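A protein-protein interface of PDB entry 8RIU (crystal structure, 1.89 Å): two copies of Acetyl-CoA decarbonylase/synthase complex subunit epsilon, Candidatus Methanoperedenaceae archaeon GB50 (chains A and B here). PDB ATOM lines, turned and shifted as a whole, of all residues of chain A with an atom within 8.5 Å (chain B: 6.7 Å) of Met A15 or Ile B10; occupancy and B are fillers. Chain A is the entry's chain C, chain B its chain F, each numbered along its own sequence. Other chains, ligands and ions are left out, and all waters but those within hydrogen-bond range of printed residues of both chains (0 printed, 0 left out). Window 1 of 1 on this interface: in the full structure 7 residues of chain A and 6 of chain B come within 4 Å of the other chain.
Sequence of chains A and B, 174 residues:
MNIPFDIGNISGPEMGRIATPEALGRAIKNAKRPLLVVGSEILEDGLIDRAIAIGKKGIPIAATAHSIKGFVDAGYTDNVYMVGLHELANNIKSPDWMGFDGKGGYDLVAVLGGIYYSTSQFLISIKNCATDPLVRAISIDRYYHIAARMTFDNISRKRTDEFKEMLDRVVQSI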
ATOM      1  N   ASN A   2       9.281 -32.544 -17.166  1.00  0.00           N
ATOM      2  CA  ASN A   2       7.889 -32.529 -17.595  1.00  0.00           C
ATOM      3  C   ASN A   2       7.702 -33.656 -18.601  1.00  0.00           C
ATOM      4  O   ASN A   2       8.425 -33.718 -19.599  1.00  0.00           O
ATOM      5  CB  ASN A   2       7.522 -31.180 -18.221  1.00  0.00           C
ATOM      6  CG  ASN A   2       7.937 -30.002 -17.359  1.00  0.00           C
ATOM      7  OD1 ASN A   2       8.582 -29.063 -17.833  1.00  0.00           O
ATOM      8  ND2 ASN A   2       7.577 -30.048 -16.086  1.00  0.00           N
ATOM      9  N   PRO A   4       5.318 -35.334 -21.298  1.00  0.00           N
ATOM     10  CA  PRO A   4       4.117 -35.305 -22.121  1.00  0.00           C
ATOM     11  C   PRO A   4       3.533 -36.727 -22.141  1.00  0.00           C
ATOM     12  O   PRO A   4       4.295 -37.657 -22.161  1.00  0.00           O
ATOM     13  CB  PRO A   4       4.613 -34.820 -23.491  1.00  0.00           C
ATOM     14  CG  PRO A   4       6.020 -34.319 -23.256  1.00  0.00           C
ATOM     15  CD  PRO A   4       6.536 -35.083 -22.057  1.00  0.00           C
ATOM     16  N   ASN A   9       5.611 -36.491 -28.323  1.00  0.00           N
ATOM     17  CA  ASN A   9       4.881 -35.259 -28.625  1.00  0.00           C
ATOM     18  C   ASN A   9       5.749 -34.050 -28.295  1.00  0.00           C
ATOM     19  O   ASN A   9       5.301 -33.126 -27.610  1.00  0.00           O
ATOM     20  CB  ASN A   9       3.581 -35.248 -27.819  1.00  0.00           C
ATOM     21  CG  ASN A   9       2.590 -34.198 -28.290  1.00  0.00           C
ATOM     22  OD1 ASN A   9       2.646 -33.723 -29.426  1.00  0.00           O
ATOM     23  ND2 ASN A   9       1.647 -33.857 -27.420  1.00  0.00           N
ATOM     24  N   ILE A  10       6.996 -34.053 -28.769  1.00  0.00           N
ATOM     25  CA  ILE A  10       7.908 -32.909 -28.653  1.00  0.00           C
ATOM     26  C   ILE A  10       7.761 -32.109 -29.946  1.00  0.00           C
ATOM     27  O   ILE A  10       8.437 -32.364 -30.956  1.00  0.00           O
ATOM     28  CB  ILE A  10       9.347 -33.353 -28.402  1.00  0.00           C
ATOM     29  CG1 ILE A  10       9.429 -34.361 -27.247  1.00  0.00           C
ATOM     30  CG2 ILE A  10      10.215 -32.163 -28.078  1.00  0.00           C
ATOM     31  CD1 ILE A  10       8.709 -33.938 -25.992  1.00  0.00           C
ATOM     32  N   SER A  11       6.875 -31.110 -29.913  1.00  0.00           N
ATOM     33  CA  SER A  11       6.414 -30.487 -31.147  1.00  0.00           C
ATOM     34  C   SER A  11       7.371 -29.426 -31.662  1.00  0.00           C
ATOM     35  O   SER A  11       7.464 -29.227 -32.875  1.00  0.00           O
ATOM     36  CB  SER A  11       5.046 -29.845 -30.930  1.00  0.00           C
ATOM     37  OG  SER A  11       5.167 -28.765 -30.012  1.00  0.00           O
ATOM     38  N   GLY A  12       8.050 -28.721 -30.764  1.00  0.00           N
ATOM     39  CA  GLY A  12       8.861 -27.587 -31.127  1.00  0.00           C
ATOM     40  C   GLY A  12       9.414 -26.879 -29.907  1.00  0.00           C
ATOM     41  O   GLY A  12       9.324 -27.369 -28.779  1.00  0.00           O
ATOM     42  N   PRO A  13       9.997 -25.696 -30.111  1.00  0.00           N
ATOM     43  CA  PRO A  13      10.722 -25.041 -29.011  1.00  0.00           C
ATOM     44  C   PRO A  13       9.859 -24.365 -27.954  1.00  0.00           C
ATOM     45  O   PRO A  13      10.359 -24.143 -26.842  1.00  0.00           O
ATOM     46  CB  PRO A  13      11.596 -24.009 -29.737  1.00  0.00           C
ATOM     47  CG  PRO A  13      10.890 -23.748 -31.032  1.00  0.00           C
ATOM     48  CD  PRO A  13      10.212 -25.028 -31.406  1.00  0.00           C
ATOM     49  N   GLU A  14       8.598 -24.048 -28.224  1.00  0.00           N
ATOM     50  CA  GLU A  14       7.776 -23.297 -27.275  1.00  0.00           C
ATOM     51  C   GLU A  14       6.890 -24.283 -26.524  1.00  0.00           C
ATOM     52  O   GLU A  14       5.832 -24.688 -27.013  1.00  0.00           O
ATOM     53  CB  GLU A  14       6.956 -22.232 -27.991  1.00  0.00           C
ATOM     54  CG  GLU A  14       6.235 -21.288 -27.044  1.00  0.00           C
ATOM     55  CD  GLU A  14       5.498 -20.187 -27.783  1.00  0.00           C
ATOM     56  OE1 GLU A  14       4.365 -20.456 -28.232  1.00  0.00           O
ATOM     57  OE2 GLU A  14       6.055 -19.073 -27.927  1.00  0.00           O
ATOM     58  N   MET A  15       7.315 -24.642 -25.318  1.00  0.00           N
ATOM     59  CA  MET A  15       6.760 -25.745 -24.550  1.00  0.00           C
ATOM     60  C   MET A  15       5.923 -25.206 -23.399  1.00  0.00           C
ATOM     61  O   MET A  15       6.316 -24.241 -22.737  1.00  0.00           O
ATOM     62  CB  MET A  15       7.899 -26.613 -24.010  1.00  0.00           C
ATOM     63  CG  MET A  15       8.833 -27.114 -25.098  1.00  0.00           C
ATOM     64  SD  MET A  15       9.758 -28.583 -24.620  1.00  0.00           S
ATOM     65  CE  MET A  15      10.786 -28.792 -26.066  1.00  0.00           C
ATOM     66  N   GLY A  16       4.781 -25.842 -23.143  1.00  0.00           N
ATOM     67  CA  GLY A  16       3.900 -25.364 -22.093  1.00  0.00           C
ATOM     68  C   GLY A  16       4.588 -25.163 -20.758  1.00  0.00           C
ATOM     69  O   GLY A  16       5.391 -25.997 -20.323  1.00  0.00           O
ATOM     70  N   ARG A  17       4.273 -24.057 -20.091  1.00  0.00           N
ATOM     71  CA  ARG A  17       4.834 -23.759 -18.781  1.00  0.00           C
ATOM     72  C   ARG A  17       4.005 -24.406 -17.679  1.00  0.00           C
ATOM     73  O   ARG A  17       2.769 -24.402 -17.726  1.00  0.00           O
ATOM     74  CB  ARG A  17       4.895 -22.247 -18.549  1.00  0.00           C
ATOM     75  CG  ARG A  17       6.144 -21.587 -19.073  1.00  0.00           C
ATOM     76  CD  ARG A  17       6.356 -21.789 -20.565  1.00  0.00           C
ATOM     77  NE  ARG A  17       7.324 -20.808 -21.041  1.00  0.00           N
ATOM     78  CZ  ARG A  17       7.784 -20.722 -22.281  1.00  0.00           C
ATOM     79  NH1 ARG A  17       7.388 -21.554 -23.230  1.00  0.00           N
ATOM     80  NH2 ARG A  17       8.678 -19.783 -22.570  1.00  0.00           N
ATOM     81  N   ILE A  18       4.697 -24.961 -16.683  1.00  0.00           N
ATOM     82  CA  ILE A  18       4.025 -25.480 -15.499  1.00  0.00           C
ATOM     83  C   ILE A  18       3.491 -24.305 -14.691  1.00  0.00           C
ATOM     84  O   ILE A  18       4.214 -23.338 -14.425  1.00  0.00           O
ATOM     85  CB  ILE A  18       4.987 -26.334 -14.659  1.00  0.00           C
ATOM     86  CG1 ILE A  18       5.544 -27.514 -15.471  1.00  0.00           C
ATOM     87  CG2 ILE A  18       4.282 -26.837 -13.402  1.00  0.00           C
ATOM     88  CD1 ILE A  18       4.501 -28.494 -15.990  1.00  0.00           C
ATOM     89  N   LYS A 127      -2.499 -22.596 -30.468  1.00  0.00           N
ATOM     90  CA  LYS A 127      -1.177 -22.014 -30.258  1.00  0.00           C
ATOM     91  C   LYS A 127      -0.608 -21.445 -31.546  1.00  0.00           C
ATOM     92  O   LYS A 127      -0.003 -20.365 -31.548  1.00  0.00           O
ATOM     93  CB  LYS A 127      -0.241 -23.085 -29.693  1.00  0.00           C
ATOM     94  CG  LYS A 127       1.232 -22.737 -29.697  1.00  0.00           C
ATOM     95  CD  LYS A 127       2.012 -23.839 -28.995  1.00  0.00           C
ATOM     96  CE  LYS A 127       3.476 -23.767 -29.293  1.00  0.00           C
ATOM     97  NZ  LYS A 127       4.089 -25.111 -29.164  1.00  0.00           N
ATOM     98  N   TYR A 144       0.519 -33.318 -18.810  1.00  0.00           N
ATOM     99  CA  TYR A 144       1.411 -32.165 -19.075  1.00  0.00           C
ATOM    100  C   TYR A 144       1.201 -31.790 -20.544  1.00  0.00           C
ATOM    101  O   TYR A 144       1.749 -32.487 -21.419  1.00  0.00           O
ATOM    102  CB  TYR A 144       2.881 -32.504 -18.828  1.00  0.00           C
ATOM    103  CG  TYR A 144       3.826 -31.531 -19.488  1.00  0.00           C
ATOM    104  CD1 TYR A 144       3.805 -30.189 -19.153  1.00  0.00           C
ATOM    105  CD2 TYR A 144       4.710 -31.938 -20.474  1.00  0.00           C
ATOM    106  CE1 TYR A 144       4.650 -29.277 -19.761  1.00  0.00           C
ATOM    107  CE2 TYR A 144       5.562 -31.039 -21.093  1.00  0.00           C
ATOM    108  CZ  TYR A 144       5.533 -29.704 -20.735  1.00  0.00           C
ATOM    109  OH  TYR A 144       6.371 -28.796 -21.336  1.00  0.00           O
ATOM    110  N   HIS A 145       0.396 -30.761 -20.804  1.00  0.00           N
ATOM    111  CA  HIS A 145       0.088 -30.384 -22.210  1.00  0.00           C
ATOM    112  C   HIS A 145       1.187 -29.452 -22.732  1.00  0.00           C
ATOM    113  O   HIS A 145       1.068 -28.218 -22.582  1.00  0.00           O
ATOM    114  CB  HIS A 145      -1.328 -29.807 -22.314  1.00  0.00           C
ATOM    115  CG  HIS A 145      -2.363 -30.847 -22.590  1.00  0.00           C
ATOM    116  ND1 HIS A 145      -2.368 -31.609 -23.737  1.00  0.00           N
ATOM    117  CD2 HIS A 145      -3.416 -31.252 -21.872  1.00  0.00           C
ATOM    118  CE1 HIS A 145      -3.398 -32.441 -23.705  1.00  0.00           C
ATOM    119  NE2 HIS A 145      -4.046 -32.241 -22.580  1.00  0.00           N
ATOM    120  N   ILE A 146       2.227 -30.035 -23.328  1.00  0.00           N
ATOM    121  CA  ILE A 146       3.363 -29.233 -23.873  1.00  0.00           C
ATOM    122  C   ILE A 146       2.828 -28.213 -24.885  1.00  0.00           C
ATOM    123  O   ILE A 146       3.488 -27.176 -25.075  1.00  0.00           O
ATOM    124  CB  ILE A 146       4.407 -30.179 -24.500  1.00  0.00           C
ATOM    125  CG1 ILE A 146       5.739 -29.476 -24.771  1.00  0.00           C
ATOM    126  CG2 ILE A 146       3.852 -30.842 -25.752  1.00  0.00           C
ATOM    127  CD1 ILE A 146       6.794 -30.386 -25.352  1.00  0.00           C
ATOM    128  N   ALA A 147       1.677 -28.494 -25.501  1.00  0.00           N
ATOM    129  CA  ALA A 147       1.113 -27.595 -26.501  1.00  0.00           C
ATOM    130  C   ALA A 147       0.245 -26.497 -25.903  1.00  0.00           C
ATOM    131  O   ALA A 147      -0.168 -25.583 -26.634  1.00  0.00           O
ATOM    132  CB  ALA A 147       0.272 -28.395 -27.501  1.00  0.00           C
ATOM    133  N   ALA A 148      -0.070 -26.578 -24.614  1.00  0.00           N
ATOM    134  CA  ALA A 148      -0.763 -25.493 -23.944  1.00  0.00           C
ATOM    135  C   ALA A 148       0.219 -24.386 -23.579  1.00  0.00           C
ATOM    136  O   ALA A 148       1.433 -24.591 -23.497  1.00  0.00           O
ATOM    137  CB  ALA A 148      -1.468 -25.986 -22.682  1.00  0.00           C
ATOM    138  N   ARG A 149      -0.330 -23.192 -23.373  1.00  0.00           N
ATOM    139  CA  ARG A 149       0.463 -22.081 -22.859  1.00  0.00           C
ATOM    140  C   ARG A 149       0.911 -22.361 -21.434  1.00  0.00           C
ATOM    141  O   ARG A 149       2.088 -22.194 -21.089  1.00  0.00           O
ATOM    142  CB  ARG A 149      -0.376 -20.805 -22.917  1.00  0.00           C
ATOM    143  CG  ARG A 149       0.381 -19.513 -22.934  1.00  0.00           C
ATOM    144  CD  ARG A 149      -0.568 -18.383 -23.298  1.00  0.00           C
ATOM    145  NE  ARG A 149       0.084 -17.086 -23.190  1.00  0.00           N
ATOM    146  CZ  ARG A 149       0.645 -16.440 -24.203  1.00  0.00           C
ATOM    147  NH1 ARG A 149       0.659 -16.945 -25.424  1.00  0.00           N
ATOM    148  NH2 ARG A 149       1.218 -15.261 -23.979  1.00  0.00           N
ATOM    149  N   MET A 150      -0.059 -22.728 -20.597  1.00  0.00           N
ATOM    150  CA  MET A 150       0.228 -23.070 -19.184  1.00  0.00           C
ATOM    151  C   MET A 150      -0.471 -24.399 -18.893  1.00  0.00           C
ATOM    152  O   MET A 150      -1.530 -24.645 -19.494  1.00  0.00           O
ATOM    153  CB  MET A 150      -0.310 -21.993 -18.242  1.00  0.00           C
ATOM    154  CG  MET A 150       0.240 -20.610 -18.519  1.00  0.00           C
ATOM    155  SD  MET A 150      -0.283 -19.413 -17.266  1.00  0.00           S
ATOM    156  CE  MET A 150      -2.050 -19.702 -17.245  1.00  0.00           C
ATOM    157  N   THR A 151       0.099 -25.216 -18.012  1.00  0.00           N
ATOM    158  CA  THR A 151      -0.475 -26.560 -17.776  1.00  0.00           C
ATOM    159  C   THR A 151       0.029 -27.157 -16.468  1.00  0.00           C
ATOM    160  O   THR A 151       0.999 -26.625 -15.912  1.00  0.00           O
ATOM    161  CB  THR A 151      -0.051 -27.527 -18.887  1.00  0.00           C
ATOM    162  OG1 THR A 151      -0.564 -28.831 -18.609  1.00  0.00           O
ATOM    163  CG2 THR A 151       1.451 -27.602 -19.049  1.00  0.00           C
ATOM    164  N   ASN B   2      16.251 -23.068 -21.244  1.00  0.00           N
ATOM    165  CA  ASN B   2      17.497 -23.464 -21.951  1.00  0.00           C
ATOM    166  C   ASN B   2      17.342 -23.129 -23.438  1.00  0.00           C
ATOM    167  O   ASN B   2      16.394 -23.639 -24.056  1.00  0.00           O
ATOM    168  CB  ASN B   2      17.835 -24.937 -21.719  1.00  0.00           C
ATOM    169  CG  ASN B   2      17.709 -25.347 -20.268  1.00  0.00           C
ATOM    170  OD1 ASN B   2      17.115 -26.377 -19.958  1.00  0.00           O
ATOM    171  ND2 ASN B   2      18.263 -24.548 -19.372  1.00  0.00           N
ATOM    172  N   PRO B   4      18.719 -23.511 -27.161  1.00  0.00           N
ATOM    173  CA  PRO B   4      19.652 -24.141 -28.093  1.00  0.00           C
ATOM    174  C   PRO B   4      20.121 -23.073 -29.091  1.00  0.00           C
ATOM    175  O   PRO B   4      19.326 -22.221 -29.427  1.00  0.00           O
ATOM    176  CB  PRO B   4      18.799 -25.232 -28.754  1.00  0.00           C
ATOM    177  CG  PRO B   4      17.379 -24.733 -28.624  1.00  0.00           C
ATOM    178  CD  PRO B   4      17.348 -24.002 -27.300  1.00  0.00           C
ATOM    179  N   ASP B   6      20.549 -23.089 -32.143  1.00  0.00           N
ATOM    180  CA  ASP B   6      19.561 -23.061 -33.243  1.00  0.00           C
ATOM    181  C   ASP B   6      18.222 -23.365 -32.568  1.00  0.00           C
ATOM    182  O   ASP B   6      18.052 -24.479 -32.083  1.00  0.00           O
ATOM    183  CB  ASP B   6      19.926 -24.022 -34.373  1.00  0.00           C
ATOM    184  CG  ASP B   6      21.112 -23.570 -35.205  1.00  0.00           C
ATOM    185  OD1 ASP B   6      21.296 -22.352 -35.350  1.00  0.00           O
ATOM    186  OD2 ASP B   6      21.832 -24.444 -35.704  1.00  0.00           O
ATOM    187  N   ILE B   7      17.344 -22.374 -32.485  1.00  0.00           N
ATOM    188  CA  ILE B   7      16.054 -22.554 -31.761  1.00  0.00           C
ATOM    189  C   ILE B   7      15.325 -23.784 -32.312  1.00  0.00           C
ATOM    190  O   ILE B   7      14.572 -24.389 -31.562  1.00  0.00           O
ATOM    191  CB  ILE B   7      15.208 -21.271 -31.855  1.00  0.00           C
ATOM    192  CG1 ILE B   7      14.036 -21.298 -30.871  1.00  0.00           C
ATOM    193  CG2 ILE B   7      14.752 -21.019 -33.283  1.00  0.00           C
ATOM    194  CD1 ILE B   7      14.441 -21.618 -29.457  1.00  0.00           C
ATOM    195  N   GLY B   8      15.562 -24.125 -33.577  1.00  0.00           N
ATOM    196  CA  GLY B   8      14.874 -25.249 -34.176  1.00  0.00           C
ATOM    197  C   GLY B   8      15.464 -26.607 -33.870  1.00  0.00           C
ATOM    198  O   GLY B   8      14.938 -27.630 -34.321  1.00  0.00           O
ATOM    199  N   ASN B   9      16.536 -26.654 -33.085  1.00  0.00           N
ATOM    200  CA  ASN B   9      17.256 -27.895 -32.833  1.00  0.00           C
ATOM    201  C   ASN B   9      16.599 -28.668 -31.693  1.00  0.00           C
ATOM    202  O   ASN B   9      17.275 -29.076 -30.747  1.00  0.00           O
ATOM    203  CB  ASN B   9      18.724 -27.572 -32.527  1.00  0.00           C
ATOM    204  CG  ASN B   9      19.622 -28.797 -32.532  1.00  0.00           C
ATOM    205  OD1 ASN B   9      19.333 -29.807 -33.178  1.00  0.00           O
ATOM    206  ND2 ASN B   9      20.738 -28.702 -31.818  1.00  0.00           N
ATOM    207  N   ILE B  10      15.284 -28.873 -31.778  1.00  0.00           N
ATOM    208  CA  ILE B  10      14.529 -29.635 -30.781  1.00  0.00           C
ATOM    209  C   ILE B  10      14.409 -31.051 -31.338  1.00  0.00           C
ATOM    210  O   ILE B  10      13.477 -31.391 -32.078  1.00  0.00           O
ATOM    211  CB  ILE B  10      13.164 -29.012 -30.484  1.00  0.00           C
ATOM    212  CG1 ILE B  10      13.272 -27.513 -30.193  1.00  0.00           C
ATOM    213  CG2 ILE B  10      12.522 -29.702 -29.278  1.00  0.00           C
ATOM    214  CD1 ILE B  10      14.267 -27.148 -29.112  1.00  0.00           C
ATOM    215  N   SER B  11      15.363 -31.897 -30.958  1.00  0.00           N
ATOM    216  CA  SER B  11      15.546 -33.169 -31.641  1.00  0.00           C
ATOM    217  C   SER B  11      14.576 -34.235 -31.158  1.00  0.00           C
ATOM    218  O   SER B  11      14.146 -35.073 -31.952  1.00  0.00           O
ATOM    219  CB  SER B  11      16.984 -33.646 -31.441  1.00  0.00           C
ATOM    220  OG  SER B  11      17.202 -33.961 -30.083  1.00  0.00           O
ATOM    221  N   GLY B  12      14.219 -34.217 -29.882  1.00  0.00           N
ATOM    222  CA  GLY B  12      13.443 -35.275 -29.285  1.00  0.00           C
ATOM    223  C   GLY B  12      13.273 -35.044 -27.800  1.00  0.00           C
ATOM    224  O   GLY B  12      13.610 -33.983 -27.271  1.00  0.00           O
ATOM    225  N   MET B  15      16.667 -34.468 -23.457  1.00  0.00           N
ATOM    226  CA  MET B  15      17.254 -33.160 -23.673  1.00  0.00           C
ATOM    227  C   MET B  15      18.409 -32.992 -22.699  1.00  0.00           C
ATOM    228  O   MET B  15      18.317 -33.431 -21.547  1.00  0.00           O
ATOM    229  CB  MET B  15      16.185 -32.092 -23.463  1.00  0.00           C
ATOM    230  CG  MET B  15      15.129 -32.124 -24.553  1.00  0.00           C
ATOM    231  SD  MET B  15      14.057 -30.675 -24.666  1.00  0.00           S
ATOM    232  CE  MET B  15      13.686 -30.318 -22.964  1.00  0.00           C
ATOM    233  N   ILE B 146      21.740 -29.368 -26.542  1.00  0.00           N
ATOM    234  CA  ILE B 146      20.579 -30.200 -26.272  1.00  0.00           C
ATOM    235  C   ILE B 146      20.840 -31.653 -26.618  1.00  0.00           C
ATOM    236  O   ILE B 146      20.150 -32.548 -26.113  1.00  0.00           O
ATOM    237  CB  ILE B 146      19.371 -29.623 -27.048  1.00  0.00           C
ATOM    238  CG1 ILE B 146      18.061 -30.174 -26.499  1.00  0.00           C
ATOM    239  CG2 ILE B 146      19.505 -29.869 -28.549  1.00  0.00           C
ATOM    240  CD1 ILE B 146      16.833 -29.489 -27.080  1.00  0.00           C
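Of the printed residues of chain B, Ile A10 touches Ile B10 and Gly B12. Of the printed residues of chain B, Gly A12 touches Ile B10. Of the printed residues of chain B, Pro A13 touches Ile B7 and Ile B10. Glu A14 touches none of the printed residues of chain B. Met A15 touches just one residue of chain B: Ile B10 (3.8 Å). Ile B10 touches four residues of chain A. No residue of chain A comes within 4 Å of Ser B11. Of the printed residues of chain A, Gly B12 touches Ile A10. Met B15 touches none of the printed residues of chain A. The nearest printed residue of chain B that does not touch Gly A12 is Ile B7 (6.0 Å).
Of the 11 printed residues of chain B, 3 touch a printed residue of chain A. Printed residues of chain B that touch a printed residue of chain A: Ile B7, Ile B10 and Gly B12. Hydrophobic or aromatic side chains of chain B that line the printed part of chain A: Ile B7 and Ile B10. Along chain B the printed residues that touch a printed residue of chain A span positions 7 to 12. Of the 21 printed residues of chain A, 4 touch a printed residue of chain B. Among the printed residues, no Asp or Glu carboxylate lies within 4 Å of a Lys or Arg side-chain nitrogen of the other chain.
The backbone carbonyl oxygen (O) of Met A15 lies within hydrogen-bond range of the guanidinium group (NH1) of Arg A17, at 2.9 Å.
CG2 of Ile B10 touches CG2 of Ile A10, at 3.6 Å. Ile A10 touches Gly B12. C of Gly A12 touches CG1 of Ile B10, 3.9 Å away. Pro A13 touches Ile B7. Pro A13 touches Ile B10 (CA to CG1, 3.7 Å). Ile B10 touches Met A15.
Ile A10 touches its own counterpart, Ile B10. Ile A10 touches Gly B12, and with the chains exchanged Gly A12 touches Ile B10. Met A15 touches Ile B10, but with the chains exchanged Ile A10 does not touch Met B15 (5.3 Å). 8 positions are printed for both chains. Of the 6 pairs that touch across the chains among the printed residues, 3 have their exchanged pair printed and touching as well.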
